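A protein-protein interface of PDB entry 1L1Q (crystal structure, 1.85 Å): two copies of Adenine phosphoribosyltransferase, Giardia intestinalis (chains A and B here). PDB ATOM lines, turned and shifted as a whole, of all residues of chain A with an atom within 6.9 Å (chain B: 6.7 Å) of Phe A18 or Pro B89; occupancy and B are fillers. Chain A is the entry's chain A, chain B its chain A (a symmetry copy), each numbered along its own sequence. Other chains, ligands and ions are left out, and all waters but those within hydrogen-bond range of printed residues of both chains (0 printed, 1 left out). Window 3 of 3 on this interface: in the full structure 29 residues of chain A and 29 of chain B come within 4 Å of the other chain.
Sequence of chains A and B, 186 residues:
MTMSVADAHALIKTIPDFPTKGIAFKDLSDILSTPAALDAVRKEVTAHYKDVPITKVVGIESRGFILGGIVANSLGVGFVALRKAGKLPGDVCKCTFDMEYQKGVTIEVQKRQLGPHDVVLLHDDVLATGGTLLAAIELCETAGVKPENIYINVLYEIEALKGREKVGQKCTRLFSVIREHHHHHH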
ATOM      1  N   ILE A  15      26.690  33.388   6.145  1.00  0.00           N
ATOM      2  CA  ILE A  15      27.369  32.578   7.153  1.00  0.00           C
ATOM      3  C   ILE A  15      28.854  32.938   7.212  1.00  0.00           C
ATOM      4  O   ILE A  15      29.581  32.755   6.233  1.00  0.00           O
ATOM      5  CB  ILE A  15      27.256  31.076   6.813  1.00  0.00           C
ATOM      6  CG1 ILE A  15      25.798  30.713   6.510  1.00  0.00           C
ATOM      7  CG2 ILE A  15      27.799  30.236   7.963  1.00  0.00           C
ATOM      8  CD1 ILE A  15      24.865  30.879   7.679  1.00  0.00           C
ATOM      9  N   PRO A  16      29.328  33.442   8.365  1.00  0.00           N
ATOM     10  CA  PRO A  16      30.740  33.814   8.501  1.00  0.00           C
ATOM     11  C   PRO A  16      31.715  32.639   8.593  1.00  0.00           C
ATOM     12  O   PRO A  16      31.375  31.572   9.099  1.00  0.00           O
ATOM     13  CB  PRO A  16      30.746  34.659   9.769  1.00  0.00           C
ATOM     14  CG  PRO A  16      29.698  33.991  10.601  1.00  0.00           C
ATOM     15  CD  PRO A  16      28.583  33.758   9.596  1.00  0.00           C
ATOM     16  N   ASP A  17      32.925  32.851   8.083  1.00  0.00           N
ATOM     17  CA  ASP A  17      33.984  31.846   8.114  1.00  0.00           C
ATOM     18  C   ASP A  17      33.562  30.460   7.638  1.00  0.00           C
ATOM     19  O   ASP A  17      33.758  29.466   8.342  1.00  0.00           O
ATOM     20  CB  ASP A  17      34.555  31.742   9.534  1.00  0.00           C
ATOM     21  CG  ASP A  17      35.059  33.075  10.060  1.00  0.00           C
ATOM     22  OD1 ASP A  17      35.936  33.676   9.403  1.00  0.00           O
ATOM     23  OD2 ASP A  17      34.581  33.519  11.130  1.00  0.00           O
ATOM     24  N   PHE A  18      32.989  30.395   6.441  1.00  0.00           N
ATOM     25  CA  PHE A  18      32.554  29.121   5.878  1.00  0.00           C
ATOM     26  C   PHE A  18      32.790  29.099   4.373  1.00  0.00           C
ATOM     27  O   PHE A  18      32.453  30.055   3.676  1.00  0.00           O
ATOM     28  CB  PHE A  18      31.068  28.890   6.141  1.00  0.00           C
ATOM     29  CG  PHE A  18      30.590  27.546   5.686  1.00  0.00           C
ATOM     30  CD1 PHE A  18      30.726  26.438   6.510  1.00  0.00           C
ATOM     31  CD2 PHE A  18      30.061  27.371   4.412  1.00  0.00           C
ATOM     32  CE1 PHE A  18      30.348  25.168   6.075  1.00  0.00           C
ATOM     33  CE2 PHE A  18      29.679  26.105   3.963  1.00  0.00           C
ATOM     34  CZ  PHE A  18      29.826  25.001   4.802  1.00  0.00           C
ATOM     35  N   PRO A  19      33.370  28.004   3.847  1.00  0.00           N
ATOM     36  CA  PRO A  19      33.807  26.799   4.563  1.00  0.00           C
ATOM     37  C   PRO A  19      35.078  27.027   5.393  1.00  0.00           C
ATOM     38  O   PRO A  19      35.290  26.373   6.413  1.00  0.00           O
ATOM     39  CB  PRO A  19      34.021  25.793   3.434  1.00  0.00           C
ATOM     40  CG  PRO A  19      34.524  26.666   2.323  1.00  0.00           C
ATOM     41  CD  PRO A  19      33.600  27.860   2.398  1.00  0.00           C
ATOM     42  N   THR A  20      35.915  27.956   4.942  1.00  0.00           N
ATOM     43  CA  THR A  20      37.153  28.287   5.636  1.00  0.00           C
ATOM     44  C   THR A  20      37.032  29.703   6.190  1.00  0.00           C
ATOM     45  O   THR A  20      36.311  30.533   5.630  1.00  0.00           O
ATOM     46  CB  THR A  20      38.367  28.211   4.679  1.00  0.00           C
ATOM     47  OG1 THR A  20      38.120  29.021   3.523  1.00  0.00           O
ATOM     48  CG2 THR A  20      38.608  26.779   4.239  1.00  0.00           C
ATOM     49  N   LYS A  21      37.727  29.978   7.290  1.00  0.00           N
ATOM     50  CA  LYS A  21      37.676  31.297   7.913  1.00  0.00           C
ATOM     51  C   LYS A  21      38.086  32.417   6.967  1.00  0.00           C
ATOM     52  O   LYS A  21      39.024  32.273   6.186  1.00  0.00           O
ATOM     53  CB  LYS A  21      38.545  31.330   9.178  1.00  0.00           C
ATOM     54  CG  LYS A  21      39.899  30.648   9.054  1.00  0.00           C
ATOM     55  CD  LYS A  21      40.658  30.743  10.376  1.00  0.00           C
ATOM     56  CE  LYS A  21      41.897  29.855  10.400  1.00  0.00           C
ATOM     57  NZ  LYS A  21      41.550  28.402  10.454  1.00  0.00           N
ATOM     58  N   GLY A  22      37.366  33.533   7.040  1.00  0.00           N
ATOM     59  CA  GLY A  22      37.658  34.665   6.182  1.00  0.00           C
ATOM     60  C   GLY A  22      36.740  34.716   4.976  1.00  0.00           C
ATOM     61  O   GLY A  22      36.773  35.671   4.199  1.00  0.00           O
ATOM     62  N   ILE A  23      35.917  33.684   4.817  1.00  0.00           N
ATOM     63  CA  ILE A  23      34.984  33.617   3.695  1.00  0.00           C
ATOM     64  C   ILE A  23      33.539  33.844   4.151  1.00  0.00           C
ATOM     65  O   ILE A  23      33.033  33.115   5.002  1.00  0.00           O
ATOM     66  CB  ILE A  23      35.065  32.233   2.974  1.00  0.00           C
ATOM     67  CG1 ILE A  23      36.425  32.061   2.289  1.00  0.00           C
ATOM     68  CG2 ILE A  23      33.946  32.113   1.938  1.00  0.00           C
ATOM     69  CD1 ILE A  23      37.609  31.955   3.241  1.00  0.00           C
ATOM     70  N   ALA A  24      32.891  34.864   3.591  1.00  0.00           N
ATOM     71  CA  ALA A  24      31.499  35.173   3.914  1.00  0.00           C
ATOM     72  C   ALA A  24      30.612  34.388   2.943  1.00  0.00           C
ATOM     73  O   ALA A  24      30.403  34.811   1.804  1.00  0.00           O
ATOM     74  CB  ALA A  24      31.248  36.669   3.762  1.00  0.00           C
ATOM     75  N   PHE A  25      30.090  33.252   3.404  1.00  0.00           N
ATOM     76  CA  PHE A  25      29.260  32.375   2.571  1.00  0.00           C
ATOM     77  C   PHE A  25      27.797  32.796   2.429  1.00  0.00           C
ATOM     78  O   PHE A  25      27.111  33.042   3.418  1.00  0.00           O
ATOM     79  CB  PHE A  25      29.319  30.943   3.122  1.00  0.00           C
ATOM     80  CG  PHE A  25      28.787  29.899   2.171  1.00  0.00           C
ATOM     81  CD1 PHE A  25      29.619  29.311   1.222  1.00  0.00           C
ATOM     82  CD2 PHE A  25      27.455  29.500   2.227  1.00  0.00           C
ATOM     83  CE1 PHE A  25      29.128  28.330   0.340  1.00  0.00           C
ATOM     84  CE2 PHE A  25      26.956  28.525   1.351  1.00  0.00           C
ATOM     85  CZ  PHE A  25      27.791  27.942   0.412  1.00  0.00           C
ATOM     86  N   LYS A  26      27.319  32.852   1.189  1.00  0.00           N
ATOM     87  CA  LYS A  26      25.935  33.228   0.921  1.00  0.00           C
ATOM     88  C   LYS A  26      25.093  31.966   0.786  1.00  0.00           C
ATOM     89  O   LYS A  26      25.194  31.242  -0.212  1.00  0.00           O
ATOM     90  CB  LYS A  26      25.846  34.062  -0.359  1.00  0.00           C
ATOM     91  CG  LYS A  26      26.586  35.387  -0.270  1.00  0.00           C
ATOM     92  CD  LYS A  26      25.993  36.293   0.791  1.00  0.00           C
ATOM     93  CE  LYS A  26      26.783  37.596   0.911  1.00  0.00           C
ATOM     94  NZ  LYS A  26      26.183  38.508   1.926  1.00  0.00           N
ATOM     95  N   ASP A  27      24.275  31.709   1.802  1.00  0.00           N
ATOM     96  CA  ASP A  27      23.411  30.529   1.831  1.00  0.00           C
ATOM     97  C   ASP A  27      22.073  30.831   1.149  1.00  0.00           C
ATOM     98  O   ASP A  27      21.232  31.540   1.705  1.00  0.00           O
ATOM     99  CB  ASP A  27      23.187  30.095   3.285  1.00  0.00           C
ATOM    100  CG  ASP A  27      22.431  28.783   3.388  1.00  0.00           C
ATOM    101  OD1 ASP A  27      22.217  28.162   2.335  1.00  0.00           O
ATOM    102  OD2 ASP A  27      22.068  28.369   4.509  1.00  0.00           O
ATOM    103  N   LEU A  28      21.881  30.280  -0.050  1.00  0.00           N
ATOM    104  CA  LEU A  28      20.663  30.501  -0.833  1.00  0.00           C
ATOM    105  C   LEU A  28      19.596  29.439  -0.614  1.00  0.00           C
ATOM    106  O   LEU A  28      18.541  29.455  -1.257  1.00  0.00           O
ATOM    107  CB  LEU A  28      21.009  30.533  -2.328  1.00  0.00           C
ATOM    108  CG  LEU A  28      22.049  31.547  -2.809  1.00  0.00           C
ATOM    109  CD1 LEU A  28      22.214  31.429  -4.309  1.00  0.00           C
ATOM    110  CD2 LEU A  28      21.609  32.938  -2.440  1.00  0.00           C
ATOM    111  N   SER A  29      19.879  28.520   0.294  1.00  0.00           N
ATOM    112  CA  SER A  29      18.997  27.407   0.593  1.00  0.00           C
ATOM    113  C   SER A  29      17.521  27.715   0.848  1.00  0.00           C
ATOM    114  O   SER A  29      16.644  26.992   0.374  1.00  0.00           O
ATOM    115  CB  SER A  29      19.565  26.633   1.789  1.00  0.00           C
ATOM    116  OG  SER A  29      18.759  25.509   2.083  1.00  0.00           O
ATOM    117  N   GLU A 100      36.928  31.667  -5.516  1.00  0.00           N
ATOM    118  CA  GLU A 100      37.109  32.316  -4.212  1.00  0.00           C
ATOM    119  C   GLU A 100      37.761  31.521  -3.076  1.00  0.00           C
ATOM    120  O   GLU A 100      38.654  32.039  -2.406  1.00  0.00           O
ATOM    121  CB  GLU A 100      35.782  32.904  -3.710  1.00  0.00           C
ATOM    122  CG  GLU A 100      35.913  33.628  -2.359  1.00  0.00           C
ATOM    123  CD  GLU A 100      34.633  34.324  -1.923  1.00  0.00           C
ATOM    124  OE1 GLU A 100      33.559  33.691  -1.995  1.00  0.00           O
ATOM    125  OE2 GLU A 100      34.700  35.500  -1.499  1.00  0.00           O
ATOM    126  N   TYR A 101      37.330  30.285  -2.839  1.00  0.00           N
ATOM    127  CA  TYR A 101      37.925  29.502  -1.757  1.00  0.00           C
ATOM    128  C   TYR A 101      38.506  28.147  -2.181  1.00  0.00           C
ATOM    129  O   TYR A 101      38.509  27.184  -1.412  1.00  0.00           O
ATOM    130  CB  TYR A 101      36.913  29.322  -0.615  1.00  0.00           C
ATOM    131  CG  TYR A 101      35.557  28.798  -1.033  1.00  0.00           C
ATOM    132  CD1 TYR A 101      35.407  27.504  -1.526  1.00  0.00           C
ATOM    133  CD2 TYR A 101      34.417  29.597  -0.921  1.00  0.00           C
ATOM    134  CE1 TYR A 101      34.153  27.011  -1.899  1.00  0.00           C
ATOM    135  CE2 TYR A 101      33.153  29.115  -1.293  1.00  0.00           C
ATOM    136  CZ  TYR A 101      33.033  27.822  -1.778  1.00  0.00           C
ATOM    137  OH  TYR A 101      31.796  27.331  -2.143  1.00  0.00           O
ATOM    138  N   GLY B  86      30.326  18.708   4.742  1.00  0.00           N
ATOM    139  CA  GLY B  86      31.175  19.849   4.454  1.00  0.00           C
ATOM    140  C   GLY B  86      30.680  20.842   3.419  1.00  0.00           C
ATOM    141  O   GLY B  86      31.229  21.937   3.305  1.00  0.00           O
ATOM    142  N   LYS B  87      29.640  20.479   2.675  1.00  0.00           N
ATOM    143  CA  LYS B  87      29.109  21.356   1.638  1.00  0.00           C
ATOM    144  C   LYS B  87      27.973  22.267   2.107  1.00  0.00           C
ATOM    145  O   LYS B  87      27.823  23.381   1.601  1.00  0.00           O
ATOM    146  CB  LYS B  87      28.666  20.511   0.445  1.00  0.00           C
ATOM    147  CG  LYS B  87      29.785  19.611  -0.067  1.00  0.00           C
ATOM    148  CD  LYS B  87      29.395  18.863  -1.323  1.00  0.00           C
ATOM    149  CE  LYS B  87      30.527  17.955  -1.786  1.00  0.00           C
ATOM    150  NZ  LYS B  87      31.785  18.723  -1.983  1.00  0.00           N
ATOM    151  N   LEU B  88      27.187  21.803   3.078  1.00  0.00           N
ATOM    152  CA  LEU B  88      26.077  22.595   3.611  1.00  0.00           C
ATOM    153  C   LEU B  88      26.476  23.354   4.873  1.00  0.00           C
ATOM    154  O   LEU B  88      27.087  22.791   5.781  1.00  0.00           O
ATOM    155  CB  LEU B  88      24.880  21.692   3.935  1.00  0.00           C
ATOM    156  CG  LEU B  88      24.150  20.980   2.790  1.00  0.00           C
ATOM    157  CD1 LEU B  88      23.247  19.892   3.362  1.00  0.00           C
ATOM    158  CD2 LEU B  88      23.335  21.992   1.976  1.00  0.00           C
ATOM    159  N   PRO B  89      26.137  24.650   4.943  1.00  0.00           N
ATOM    160  CA  PRO B  89      26.455  25.489   6.105  1.00  0.00           C
ATOM    161  C   PRO B  89      25.311  25.481   7.124  1.00  0.00           C
ATOM    162  O   PRO B  89      24.208  25.027   6.820  1.00  0.00           O
ATOM    163  CB  PRO B  89      26.637  26.861   5.480  1.00  0.00           C
ATOM    164  CG  PRO B  89      25.529  26.862   4.455  1.00  0.00           C
ATOM    165  CD  PRO B  89      25.650  25.478   3.823  1.00  0.00           C
ATOM    166  N   GLY B  90      25.570  25.990   8.325  1.00  0.00           N
ATOM    167  CA  GLY B  90      24.536  26.021   9.347  1.00  0.00           C
ATOM    168  C   GLY B  90      24.358  24.696  10.062  1.00  0.00           C
ATOM    169  O   GLY B  90      25.125  23.762   9.831  1.00  0.00           O
ATOM    170  N   ASP B  91      23.347  24.609  10.924  1.00  0.00           N
ATOM    171  CA  ASP B  91      23.083  23.384  11.675  1.00  0.00           C
ATOM    172  C   ASP B  91      22.657  22.266  10.740  1.00  0.00           C
ATOM    173  O   ASP B  91      21.779  22.450   9.898  1.00  0.00           O
ATOM    174  CB  ASP B  91      22.003  23.625  12.733  1.00  0.00           C
ATOM    175  CG  ASP B  91      22.441  24.623  13.787  1.00  0.00           C
ATOM    176  OD1 ASP B  91      23.613  24.567  14.203  1.00  0.00           O
ATOM    177  OD2 ASP B  91      21.617  25.457  14.207  1.00  0.00           O
ATOM    178  N   VAL B  92      23.266  21.097  10.913  1.00  0.00           N
ATOM    179  CA  VAL B  92      22.994  19.972  10.044  1.00  0.00           C
ATOM    180  C   VAL B  92      22.869  18.621  10.749  1.00  0.00           C
ATOM    181  O   VAL B  92      23.392  18.427  11.846  1.00  0.00           O
ATOM    182  CB  VAL B  92      24.122  19.874   8.993  1.00  0.00           C
ATOM    183  CG1 VAL B  92      24.017  18.595   8.224  1.00  0.00           C
ATOM    184  CG2 VAL B  92      24.069  21.069   8.061  1.00  0.00           C
ATOM    185  N   GLU B 108      24.585  14.914   4.609  1.00  0.00           N
ATOM    186  CA  GLU B 108      24.043  15.887   5.536  1.00  0.00           C
ATOM    187  C   GLU B 108      22.839  16.620   4.975  1.00  0.00           C
ATOM    188  O   GLU B 108      22.649  16.684   3.763  1.00  0.00           O
ATOM    189  CB  GLU B 108      25.099  16.922   5.883  1.00  0.00           C
ATOM    190  CG  GLU B 108      26.394  16.356   6.422  1.00  0.00           C
ATOM    191  CD  GLU B 108      27.339  17.455   6.839  1.00  0.00           C
ATOM    192  OE1 GLU B 108      27.411  18.462   6.110  1.00  0.00           O
ATOM    193  OE2 GLU B 108      28.009  17.315   7.886  1.00  0.00           O
ATOM    194  N   GLN B 110      20.355  20.265   6.103  1.00  0.00           N
ATOM    195  CA  GLN B 110      20.211  21.378   7.043  1.00  0.00           C
ATOM    196  C   GLN B 110      19.014  21.077   7.945  1.00  0.00           C
ATOM    197  O   GLN B 110      17.908  20.847   7.458  1.00  0.00           O
ATOM    198  CB  GLN B 110      19.986  22.706   6.299  1.00  0.00           C
ATOM    199  CG  GLN B 110      21.260  23.334   5.726  1.00  0.00           C
ATOM    200  CD  GLN B 110      21.027  24.689   5.053  1.00  0.00           C
ATOM    201  OE1 GLN B 110      21.948  25.499   4.936  1.00  0.00           O
ATOM    202  NE2 GLN B 110      19.803  24.934   4.604  1.00  0.00           N
ATOM    203  N   ARG B 112      16.996  22.848   9.757  1.00  0.00           N
ATOM    204  CA  ARG B 112      15.817  23.692   9.594  1.00  0.00           C
ATOM    205  C   ARG B 112      14.934  23.412   8.375  1.00  0.00           C
ATOM    206  O   ARG B 112      13.802  23.879   8.327  1.00  0.00           O
ATOM    207  CB  ARG B 112      16.235  25.165   9.547  1.00  0.00           C
ATOM    208  CG  ARG B 112      16.955  25.594   8.251  1.00  0.00           C
ATOM    209  CD  ARG B 112      17.084  27.120   8.230  1.00  0.00           C
ATOM    210  NE  ARG B 112      17.663  27.670   7.009  1.00  0.00           N
ATOM    211  CZ  ARG B 112      18.966  27.747   6.746  1.00  0.00           C
ATOM    212  NH1 ARG B 112      19.855  27.300   7.617  1.00  0.00           N
ATOM    213  NH2 ARG B 112      19.384  28.297   5.615  1.00  0.00           N
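Hydrophobic or aromatic side chains of chain B within 4 Å of the printed part of chain A: Pro B89. Hydrophobic or aromatic side chains of chain A within 4 Å of the printed part of chain B: Phe A18 and Phe A25. Among the printed residues, Asp or Glu carboxylates within 4 Å of a Lys or Arg side-chain nitrogen of the other chain: Asp A27 with Arg B112.
OD2 of Asp A27 lies close to OE1 of Gln B110 (2.9 Å). The guanidinium group of Arg B112 is in salt-bridge range of the side-chain carboxylate of Asp A27, 2.9 Å away. The side-chain hydroxyl of Ser A29 sits at hydrogen-bond distance from the side-chain amide nitrogen of Gln B110.
Among the printed residues, merely in contact across the chains: Phe A18 with Gly B86, Phe A18 with Leu B88, Phe A18 with Pro B89, Phe A25 with Pro B89 and Asp A27 with Pro B89.
Of the printed residues of chain B, Ser A29 touches Gln B110. Of the printed residues of chain A, Leu B88 touches Phe A18 (3.7 Å). Of the printed residues of chain A, Gly B86 touches Phe A18 (3.7 Å). Of the printed residues of chain A, Arg B112 touches Asp A27 (2.9 Å). Of the printed residues of chain B, Phe A25 touches Pro B89. Gly A22 touches none of the printed residues of chain B. Leu A28 touches none of the printed residues of chain B. The nearest residue of chain A that does not touch Pro B89 is Ile A15 (4.1 Å).
The backbone NH of Ile A15 is in hydrogen-bond range of the backbone carbonyl oxygen of Phe A25 (2.8 Å). The backbone NH (N) of Phe A18 sits at hydrogen-bond distance from the backbone carbonyl oxygen (O) of Ile A23 (3.1 Å). OD1 of Asp A27 sits close to N of Ser A29, 3.1 Å away. OE1 of Glu B108 sits at hydrogen-bond distance from N of Gly B86, at 3.2 Å. The backbone carbonyl oxygen (O) of Pro B89 lies close to the side-chain amide oxygen (OE1) of Gln B110, at 3.0 Å.
No position is printed for both chains. Of the 8 pairs that touch across the chains among the printed residues, none has its exchanged pair printed and touching as well.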
